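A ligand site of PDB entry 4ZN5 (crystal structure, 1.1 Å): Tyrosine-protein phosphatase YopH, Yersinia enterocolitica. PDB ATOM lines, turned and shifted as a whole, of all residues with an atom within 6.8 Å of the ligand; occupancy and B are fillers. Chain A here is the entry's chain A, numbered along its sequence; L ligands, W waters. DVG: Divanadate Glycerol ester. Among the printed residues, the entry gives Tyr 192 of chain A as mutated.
A vanadium atom (V06) of the ligand is bound by the side-chain sulfur (SG) of Cys 241, 2.5 Å away.
N of Arg 242 lies close to O08 of the ligand (2.7 Å).
The side-chain amide nitrogen of Gln 284 is in hydrogen-bond range of an oxygen (O1) of the ligand, at 2.9 Å.
The side-chain sulfur (SG) of Cys 241 sits close to the backbone NH (N) of Gly 244 (3.4 Å).
The backbone NH (N) of Cys 241 is in hydrogen-bond range of the side-chain hydroxyl (OG1) of Thr 248, at 3.0 Å.
NH1 of Arg 247 lies within salt-bridge range of OE1 of Glu 128 (2.7 Å).
The guanidinium group (NH1) of Arg 247 is in hydrogen-bond range of the backbone carbonyl oxygen (O) of Leu 123 (2.9 Å).
The side-chain amide oxygen of Gln 288 lies within hydrogen-bond range of the backbone NH of Gln 284, 3.0 Å away.
The backbone NH (N) of Lys 285 sits at hydrogen-bond distance from the side-chain amide oxygen (OE1) of Gln 288 (2.9 Å).
The backbone NH of Gln 284 sits at hydrogen-bond distance from the backbone carbonyl oxygen of Val 245 (3.5 Å).
The backbone NH (N) of Val 283 sits at hydrogen-bond distance from the backbone carbonyl oxygen (O) of Val 245, at 2.8 Å.
The backbone NH (N) of Ala 243 sits close to an oxygen (O08) of the ligand (3.1 Å).
The backbone NH of Gly 244 lies close to an oxygen (O07) of the ligand (3.3 Å).
The backbone NH (N) of Val 245 sits close to an oxygen (O07) of the ligand.
An oxygen (O07) of the ligand sits close to the backbone NH (N) of Gly 246.
N of Arg 247 sits close to O09 of the ligand (2.8 Å).
NZ of Lys 285 sits close to O3 of the ligand, 3.0 Å away.
An oxygen (O01) of the ligand lies close to the side-chain amide nitrogen of Gln 288 (2.9 Å).
Hydrophobic or aromatic side chains that line the ligand: Ala 243 and Val 245.
Ten residues have an atom within 4 Å of the ligand: Cys 241, Arg 242, Ala 243, Gly 244, Val 245, Gly 246, Arg 247, Gln 284, Lys 285 and Gln 288.
Water W2 lies within hydrogen-bond range of O of Asp 194 and NH2 of Arg 247.
Water W4 bridges the side-chain amino group of Lys 285 (2.8 Å) and the backbone carbonyl oxygen of Asp 194 (3.1 Å).
Water W1 lies within hydrogen-bond range of the backbone carbonyl oxygen of Pro 193 (2.7 Å), the backbone carbonyl oxygen of Thr 196 (2.7 Å) and the guanidinium group of Arg 247 (3.3 Å).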
ATOM      1  N   PHE A  67     -34.142 -10.039  19.390  1.00  0.00           N
ATOM      2  CA  PHE A  67     -35.279 -10.902  19.102  1.00  0.00           C
ATOM      3  C   PHE A  67     -36.072 -11.096  20.379  1.00  0.00           C
ATOM      4  O   PHE A  67     -35.535 -11.508  21.401  1.00  0.00           O
ATOM      5  CB  PHE A  67     -34.790 -12.257  18.572  1.00  0.00           C
ATOM      6  CG  PHE A  67     -33.935 -12.144  17.359  1.00  0.00           C
ATOM      7  CD1 PHE A  67     -34.511 -11.918  16.115  1.00  0.00           C
ATOM      8  CD2 PHE A  67     -32.554 -12.222  17.440  1.00  0.00           C
ATOM      9  CE1 PHE A  67     -33.720 -11.797  14.992  1.00  0.00           C
ATOM     10  CE2 PHE A  67     -31.768 -12.108  16.313  1.00  0.00           C
ATOM     11  CZ  PHE A  67     -32.351 -11.889  15.089  1.00  0.00           C
ATOM     12  N   ILE A  70     -35.675 -14.339  22.404  1.00  0.00           N
ATOM     13  CA  ILE A  70     -34.315 -14.808  22.651  1.00  0.00           C
ATOM     14  C   ILE A  70     -33.694 -13.948  23.742  1.00  0.00           C
ATOM     15  O   ILE A  70     -33.144 -12.879  23.480  1.00  0.00           O
ATOM     16  CB  ILE A  70     -33.487 -14.798  21.366  1.00  0.00           C
ATOM     17  CG1 ILE A  70     -34.215 -15.583  20.279  1.00  0.00           C
ATOM     18  CG2 ILE A  70     -32.098 -15.350  21.650  1.00  0.00           C
ATOM     19  CD1 ILE A  70     -33.462 -15.814  19.013  1.00  0.00           C
ATOM     20  N   LEU A 123     -20.093 -14.914  13.475  1.00  0.00           N
ATOM     21  CA  LEU A 123     -20.583 -15.968  12.607  1.00  0.00           C
ATOM     22  C   LEU A 123     -21.779 -15.534  11.761  1.00  0.00           C
ATOM     23  O   LEU A 123     -22.311 -16.338  11.009  1.00  0.00           O
ATOM     24  CB  LEU A 123     -20.958 -17.198  13.432  1.00  0.00           C
ATOM     25  CG  LEU A 123     -19.884 -17.673  14.411  1.00  0.00           C
ATOM     26  CD1 LEU A 123     -20.363 -18.923  15.141  1.00  0.00           C
ATOM     27  CD2 LEU A 123     -18.564 -17.912  13.728  1.00  0.00           C
ATOM     28  N   ALA A 124     -22.189 -14.261  11.882  1.00  0.00           N
ATOM     29  CA  ALA A 124     -23.095 -13.632  10.921  1.00  0.00           C
ATOM     30  C   ALA A 124     -22.297 -13.295   9.673  1.00  0.00           C
ATOM     31  O   ALA A 124     -21.185 -12.779   9.765  1.00  0.00           O
ATOM     32  CB  ALA A 124     -23.695 -12.384  11.518  1.00  0.00           C
ATOM     33  N   GLU A 128     -25.532 -11.016   5.539  1.00  0.00           N
ATOM     34  CA  GLU A 128     -26.450 -10.690   6.608  1.00  0.00           C
ATOM     35  C   GLU A 128     -26.177  -9.278   7.121  1.00  0.00           C
ATOM     36  O   GLU A 128     -27.086  -8.484   7.309  1.00  0.00           O
ATOM     37  CB  GLU A 128     -26.356 -11.727   7.717  1.00  0.00           C
ATOM     38  CG  GLU A 128     -26.946 -13.066   7.334  1.00  0.00           C
ATOM     39  CD  GLU A 128     -26.686 -14.121   8.384  1.00  0.00           C
ATOM     40  OE1 GLU A 128     -25.542 -14.388   8.739  1.00  0.00           O
ATOM     41  OE2 GLU A 128     -27.652 -14.713   8.885  1.00  0.00           O
ATOM     42  N   TYR A 192     -20.349 -17.512   5.994  1.00  0.00           N
ATOM     43  CA  TYR A 192     -21.100 -18.530   6.709  1.00  0.00           C
ATOM     44  C   TYR A 192     -22.469 -18.620   6.024  1.00  0.00           C
ATOM     45  O   TYR A 192     -23.144 -17.604   5.859  1.00  0.00           O
ATOM     46  CB  TYR A 192     -21.279 -18.134   8.176  1.00  0.00           C
ATOM     47  CG  TYR A 192     -21.502 -19.299   9.123  1.00  0.00           C
ATOM     48  CD1 TYR A 192     -22.596 -20.142   8.985  1.00  0.00           C
ATOM     49  CD2 TYR A 192     -20.630 -19.544  10.168  1.00  0.00           C
ATOM     50  CE1 TYR A 192     -22.782 -21.202   9.845  1.00  0.00           C
ATOM     51  CE2 TYR A 192     -20.823 -20.591  11.036  1.00  0.00           C
ATOM     52  CZ  TYR A 192     -21.905 -21.419  10.882  1.00  0.00           C
ATOM     53  OH  TYR A 192     -22.059 -22.457  11.780  1.00  0.00           O
ATOM     54  N   PRO A 193     -22.907 -19.820   5.634  1.00  0.00           N
ATOM     55  CA  PRO A 193     -24.252 -19.927   5.045  1.00  0.00           C
ATOM     56  C   PRO A 193     -25.352 -19.558   6.057  1.00  0.00           C
ATOM     57  O   PRO A 193     -25.229 -19.821   7.246  1.00  0.00           O
ATOM     58  CB  PRO A 193     -24.333 -21.401   4.635  1.00  0.00           C
ATOM     59  CG  PRO A 193     -23.356 -22.102   5.513  1.00  0.00           C
ATOM     60  CD  PRO A 193     -22.217 -21.121   5.711  1.00  0.00           C
ATOM     61  N   ASP A 194     -26.437 -18.960   5.593  1.00  0.00           N
ATOM     62  CA  ASP A 194     -27.536 -18.665   6.517  1.00  0.00           C
ATOM     63  C   ASP A 194     -28.686 -19.657   6.425  1.00  0.00           C
ATOM     64  O   ASP A 194     -29.553 -19.710   7.308  1.00  0.00           O
ATOM     65  CB  ASP A 194     -28.050 -17.228   6.336  1.00  0.00           C
ATOM     66  CG  ASP A 194     -28.473 -16.946   4.919  1.00  0.00           C
ATOM     67  OD1 ASP A 194     -27.587 -16.821   4.051  1.00  0.00           O
ATOM     68  OD2 ASP A 194     -29.701 -16.819   4.678  1.00  0.00           O
ATOM     69  N   GLN A 195     -28.687 -20.476   5.382  1.00  0.00           N
ATOM     70  CA  GLN A 195     -29.809 -21.386   5.159  1.00  0.00           C
ATOM     71  C   GLN A 195     -29.476 -22.821   5.566  1.00  0.00           C
ATOM     72  O   GLN A 195     -30.375 -23.642   5.738  1.00  0.00           O
ATOM     73  CB  GLN A 195     -30.208 -21.374   3.686  1.00  0.00           C
ATOM     74  CG  GLN A 195     -30.585 -19.994   3.167  1.00  0.00           C
ATOM     75  CD  GLN A 195     -30.751 -19.976   1.651  1.00  0.00           C
ATOM     76  OE1 GLN A 195     -30.056 -20.680   0.932  1.00  0.00           O
ATOM     77  NE2 GLN A 195     -31.691 -19.163   1.173  1.00  0.00           N
ATOM     78  N   THR A 196     -28.196 -23.120   5.709  1.00  0.00           N
ATOM     79  CA  THR A 196     -27.748 -24.471   5.965  1.00  0.00           C
ATOM     80  C   THR A 196     -26.641 -24.455   7.017  1.00  0.00           C
ATOM     81  O   THR A 196     -26.040 -23.418   7.271  1.00  0.00           O
ATOM     82  CB  THR A 196     -27.224 -25.121   4.674  1.00  0.00           C
ATOM     83  OG1 THR A 196     -26.106 -24.369   4.178  1.00  0.00           O
ATOM     84  CG2 THR A 196     -28.311 -25.158   3.612  1.00  0.00           C
ATOM     85  N   ALA A 197     -26.393 -25.610   7.636  1.00  0.00           N
ATOM     86  CA  ALA A 197     -25.343 -25.739   8.631  1.00  0.00           C
ATOM     87  C   ALA A 197     -24.022 -26.027   7.962  1.00  0.00           C
ATOM     88  O   ALA A 197     -23.975 -26.702   6.942  1.00  0.00           O
ATOM     89  CB  ALA A 197     -25.671 -26.843   9.582  1.00  0.00           C
ATOM     90  N   HIS A 240     -20.639 -14.551  18.620  1.00  0.00           N
ATOM     91  CA  HIS A 240     -22.002 -14.263  18.243  1.00  0.00           C
ATOM     92  C   HIS A 240     -22.239 -14.473  16.763  1.00  0.00           C
ATOM     93  O   HIS A 240     -21.326 -14.339  15.941  1.00  0.00           O
ATOM     94  CB  HIS A 240     -22.469 -12.834  18.638  1.00  0.00           C
ATOM     95  CG  HIS A 240     -21.823 -11.693  17.889  1.00  0.00           C
ATOM     96  ND1 HIS A 240     -22.268 -11.257  16.659  1.00  0.00           N
ATOM     97  CD2 HIS A 240     -20.848 -10.817  18.264  1.00  0.00           C
ATOM     98  CE1 HIS A 240     -21.569 -10.179  16.311  1.00  0.00           C
ATOM     99  NE2 HIS A 240     -20.701  -9.904  17.259  1.00  0.00           N
ATOM    100  N   CYS A 241     -23.483 -14.795  16.448  1.00  0.00           N
ATOM    101  CA  CYS A 241     -24.030 -14.748  15.101  1.00  0.00           C
ATOM    102  C   CYS A 241     -25.014 -13.567  15.084  1.00  0.00           C
ATOM    103  O   CYS A 241     -24.595 -12.453  15.435  1.00  0.00           O
ATOM    104  CB  CYS A 241     -24.601 -16.115  14.695  1.00  0.00           C
ATOM    105  SG  CYS A 241     -25.574 -16.987  15.961  1.00  0.00           S
ATOM    106  N   ARG A 242     -26.258 -13.778  14.693  1.00  0.00           N
ATOM    107  CA  ARG A 242     -27.264 -12.713  14.813  1.00  0.00           C
ATOM    108  C   ARG A 242     -27.899 -12.772  16.200  1.00  0.00           C
ATOM    109  O   ARG A 242     -27.904 -11.792  16.944  1.00  0.00           O
ATOM    110  CB  ARG A 242     -28.331 -12.836  13.730  1.00  0.00           C
ATOM    111  CG  ARG A 242     -27.795 -12.745  12.339  1.00  0.00           C
ATOM    112  CD  ARG A 242     -28.900 -12.824  11.302  1.00  0.00           C
ATOM    113  NE  ARG A 242     -30.022 -11.954  11.626  1.00  0.00           N
ATOM    114  CZ  ARG A 242     -31.305 -12.234  11.357  1.00  0.00           C
ATOM    115  NH1 ARG A 242     -31.628 -13.367  10.750  1.00  0.00           N
ATOM    116  NH2 ARG A 242     -32.247 -11.366  11.671  1.00  0.00           N
ATOM    117  N   ALA A 243     -28.446 -13.937  16.555  1.00  0.00           N
ATOM    118  CA  ALA A 243     -29.122 -14.135  17.834  1.00  0.00           C
ATOM    119  C   ALA A 243     -28.208 -14.703  18.917  1.00  0.00           C
ATOM    120  O   ALA A 243     -28.535 -14.604  20.089  1.00  0.00           O
ATOM    121  CB  ALA A 243     -30.335 -15.038  17.667  1.00  0.00           C
ATOM    122  N   GLY A 244     -27.090 -15.320  18.536  1.00  0.00           N
ATOM    123  CA  GLY A 244     -26.217 -15.921  19.535  1.00  0.00           C
ATOM    124  C   GLY A 244     -26.729 -17.197  20.162  1.00  0.00           C
ATOM    125  O   GLY A 244     -26.359 -17.489  21.306  1.00  0.00           O
ATOM    126  N   VAL A 245     -27.518 -17.966  19.410  1.00  0.00           N
ATOM    127  CA  VAL A 245     -28.035 -19.224  19.916  1.00  0.00           C
ATOM    128  C   VAL A 245     -27.880 -20.418  18.976  1.00  0.00           C
ATOM    129  O   VAL A 245     -28.044 -21.555  19.418  1.00  0.00           O
ATOM    130  CB  VAL A 245     -29.527 -19.119  20.335  1.00  0.00           C
ATOM    131  CG1 VAL A 245     -29.689 -18.138  21.491  1.00  0.00           C
ATOM    132  CG2 VAL A 245     -30.425 -18.744  19.166  1.00  0.00           C
ATOM    133  N   GLY A 246     -27.575 -20.188  17.707  1.00  0.00           N
ATOM    134  CA  GLY A 246     -27.548 -21.266  16.726  1.00  0.00           C
ATOM    135  C   GLY A 246     -26.120 -21.585  16.334  1.00  0.00           C
ATOM    136  O   GLY A 246     -25.470 -22.438  16.939  1.00  0.00           O
ATOM    137  N   ARG A 247     -25.626 -20.881  15.328  1.00  0.00           N
ATOM    138  CA  ARG A 247     -24.247 -21.053  14.908  1.00  0.00           C
ATOM    139  C   ARG A 247     -23.299 -20.881  16.101  1.00  0.00           C
ATOM    140  O   ARG A 247     -22.295 -21.598  16.232  1.00  0.00           O
ATOM    141  CB  ARG A 247     -23.890 -20.037  13.814  1.00  0.00           C
ATOM    142  CG  ARG A 247     -24.800 -20.103  12.600  1.00  0.00           C
ATOM    143  CD  ARG A 247     -24.589 -18.901  11.720  1.00  0.00           C
ATOM    144  NE  ARG A 247     -25.729 -18.714  10.832  1.00  0.00           N
ATOM    145  CZ  ARG A 247     -25.925 -17.654  10.076  1.00  0.00           C
ATOM    146  NH1 ARG A 247     -25.023 -16.673  10.072  1.00  0.00           N
ATOM    147  NH2 ARG A 247     -27.006 -17.561   9.326  1.00  0.00           N
ATOM    148  N   THR A 248     -23.610 -19.921  16.957  1.00  0.00           N
ATOM    149  CA  THR A 248     -22.821 -19.647  18.150  1.00  0.00           C
ATOM    150  C   THR A 248     -22.720 -20.868  19.049  1.00  0.00           C
ATOM    151  O   THR A 248     -21.641 -21.189  19.557  1.00  0.00           O
ATOM    152  CB  THR A 248     -23.463 -18.473  18.907  1.00  0.00           C
ATOM    153  OG1 THR A 248     -23.253 -17.274  18.154  1.00  0.00           O
ATOM    154  CG2 THR A 248     -22.889 -18.278  20.273  1.00  0.00           C
ATOM    155  N   ALA A 249     -23.841 -21.544  19.272  1.00  0.00           N
ATOM    156  CA  ALA A 249     -23.851 -22.713  20.146  1.00  0.00           C
ATOM    157  C   ALA A 249     -23.152 -23.916  19.513  1.00  0.00           C
ATOM    158  O   ALA A 249     -22.509 -24.696  20.213  1.00  0.00           O
ATOM    159  CB  ALA A 249     -25.303 -23.061  20.524  1.00  0.00           C
ATOM    160  N   ILE A 281     -32.966 -21.844  23.859  1.00  0.00           N
ATOM    161  CA  ILE A 281     -32.830 -21.986  22.406  1.00  0.00           C
ATOM    162  C   ILE A 281     -31.422 -22.404  22.000  1.00  0.00           C
ATOM    163  O   ILE A 281     -31.210 -22.768  20.841  1.00  0.00           O
ATOM    164  CB  ILE A 281     -33.239 -20.655  21.683  1.00  0.00           C
ATOM    165  CG1 ILE A 281     -34.578 -20.138  22.233  1.00  0.00           C
ATOM    166  CG2 ILE A 281     -33.343 -20.840  20.205  1.00  0.00           C
ATOM    167  CD1 ILE A 281     -35.682 -21.163  22.166  1.00  0.00           C
ATOM    168  N   VAL A 283     -28.367 -24.022  20.681  1.00  0.00           N
ATOM    169  CA  VAL A 283     -28.443 -25.082  19.682  1.00  0.00           C
ATOM    170  C   VAL A 283     -29.870 -25.063  19.142  1.00  0.00           C
ATOM    171  O   VAL A 283     -30.725 -25.861  19.529  1.00  0.00           O
ATOM    172  CB  VAL A 283     -28.000 -26.484  20.152  1.00  0.00           C
ATOM    173  CG1 VAL A 283     -27.878 -27.383  18.951  1.00  0.00           C
ATOM    174  CG2 VAL A 283     -26.679 -26.415  20.888  1.00  0.00           C
ATOM    175  N   GLN A 284     -30.108 -24.107  18.264  1.00  0.00           N
ATOM    176  CA  GLN A 284     -31.439 -23.720  17.862  1.00  0.00           C
ATOM    177  C   GLN A 284     -32.069 -24.717  16.905  1.00  0.00           C
ATOM    178  O   GLN A 284     -33.269 -24.941  16.959  1.00  0.00           O
ATOM    179  CB  GLN A 284     -31.374 -22.324  17.209  1.00  0.00           C
ATOM    180  CG  GLN A 284     -32.700 -21.789  16.758  1.00  0.00           C
ATOM    181  CD  GLN A 284     -32.737 -20.305  16.510  1.00  0.00           C
ATOM    182  OE1 GLN A 284     -33.700 -19.634  16.886  1.00  0.00           O
ATOM    183  NE2 GLN A 284     -31.704 -19.765  15.872  1.00  0.00           N
ATOM    184  N   LYS A 285     -31.237 -25.322  16.053  1.00  0.00           N
ATOM    185  CA  LYS A 285     -31.731 -26.123  14.935  1.00  0.00           C
ATOM    186  C   LYS A 285     -31.195 -27.555  15.031  1.00  0.00           C
ATOM    187  O   LYS A 285     -30.072 -27.807  15.458  1.00  0.00           O
ATOM    188  CB  LYS A 285     -31.274 -25.473  13.616  1.00  0.00           C
ATOM    189  CG  LYS A 285     -31.824 -24.050  13.458  1.00  0.00           C
ATOM    190  CD  LYS A 285     -31.451 -23.338  12.162  1.00  0.00           C
ATOM    191  CE  LYS A 285     -32.216 -22.004  12.075  1.00  0.00           C
ATOM    192  NZ  LYS A 285     -31.948 -21.215  10.848  1.00  0.00           N
ATOM    193  N   GLN A 288     -27.803 -28.281  13.627  1.00  0.00           N
ATOM    194  CA  GLN A 288     -26.678 -27.917  14.473  1.00  0.00           C
ATOM    195  C   GLN A 288     -26.398 -29.016  15.501  1.00  0.00           C
ATOM    196  O   GLN A 288     -25.243 -29.378  15.725  1.00  0.00           O
ATOM    197  CB  GLN A 288     -26.973 -26.581  15.147  1.00  0.00           C
ATOM    198  CG  GLN A 288     -27.089 -25.448  14.160  1.00  0.00           C
ATOM    199  CD  GLN A 288     -27.907 -24.273  14.661  1.00  0.00           C
ATOM    200  OE1 GLN A 288     -28.501 -24.320  15.736  1.00  0.00           O
ATOM    201  NE2 GLN A 288     -27.933 -23.224  13.874  1.00  0.00           N
HETATM  202  O3  DVG L   1     -30.307 -19.056  12.014  1.00  0.00           O
HETATM  203  C3  DVG L   1     -31.227 -18.125  12.523  1.00  0.00           C
HETATM  204  C2  DVG L   1     -30.403 -17.154  13.353  1.00  0.00           C
HETATM  205  O2  DVG L   1     -29.593 -17.968  14.163  1.00  0.00           O
HETATM  206  C1  DVG L   1     -31.268 -16.239  14.202  1.00  0.00           C
HETATM  207  O1  DVG L   1     -32.095 -16.971  15.059  1.00  0.00           O
HETATM  208  O01 DVG L   1     -29.601 -20.878  14.157  1.00  0.00           O
HETATM  209  V02 DVG L   1     -28.933 -19.627  13.259  1.00  0.00           V
HETATM  210  O03 DVG L   1     -28.022 -20.452  11.882  1.00  0.00           O
HETATM  211  V06 DVG L   1     -27.859 -17.501  15.034  1.00  0.00           V
HETATM  212  O07 DVG L   1     -28.396 -17.627  16.655  1.00  0.00           O
HETATM  213  O08 DVG L   1     -27.878 -15.900  14.223  1.00  0.00           O
HETATM  214  O09 DVG L   1     -27.360 -19.037  14.141  1.00  0.00           O
HETATM  215  O   HOH W   1     -26.575 -21.381   9.002  1.00  0.00           O
HETATM  216  O   HOH W   2     -29.954 -18.182   9.598  1.00  0.00           O
HETATM  217  O   HOH W   3     -26.562 -23.272  11.143  1.00  0.00           O
HETATM  218  O   HOH W   4     -29.361 -21.534   9.822  1.00  0.00           O
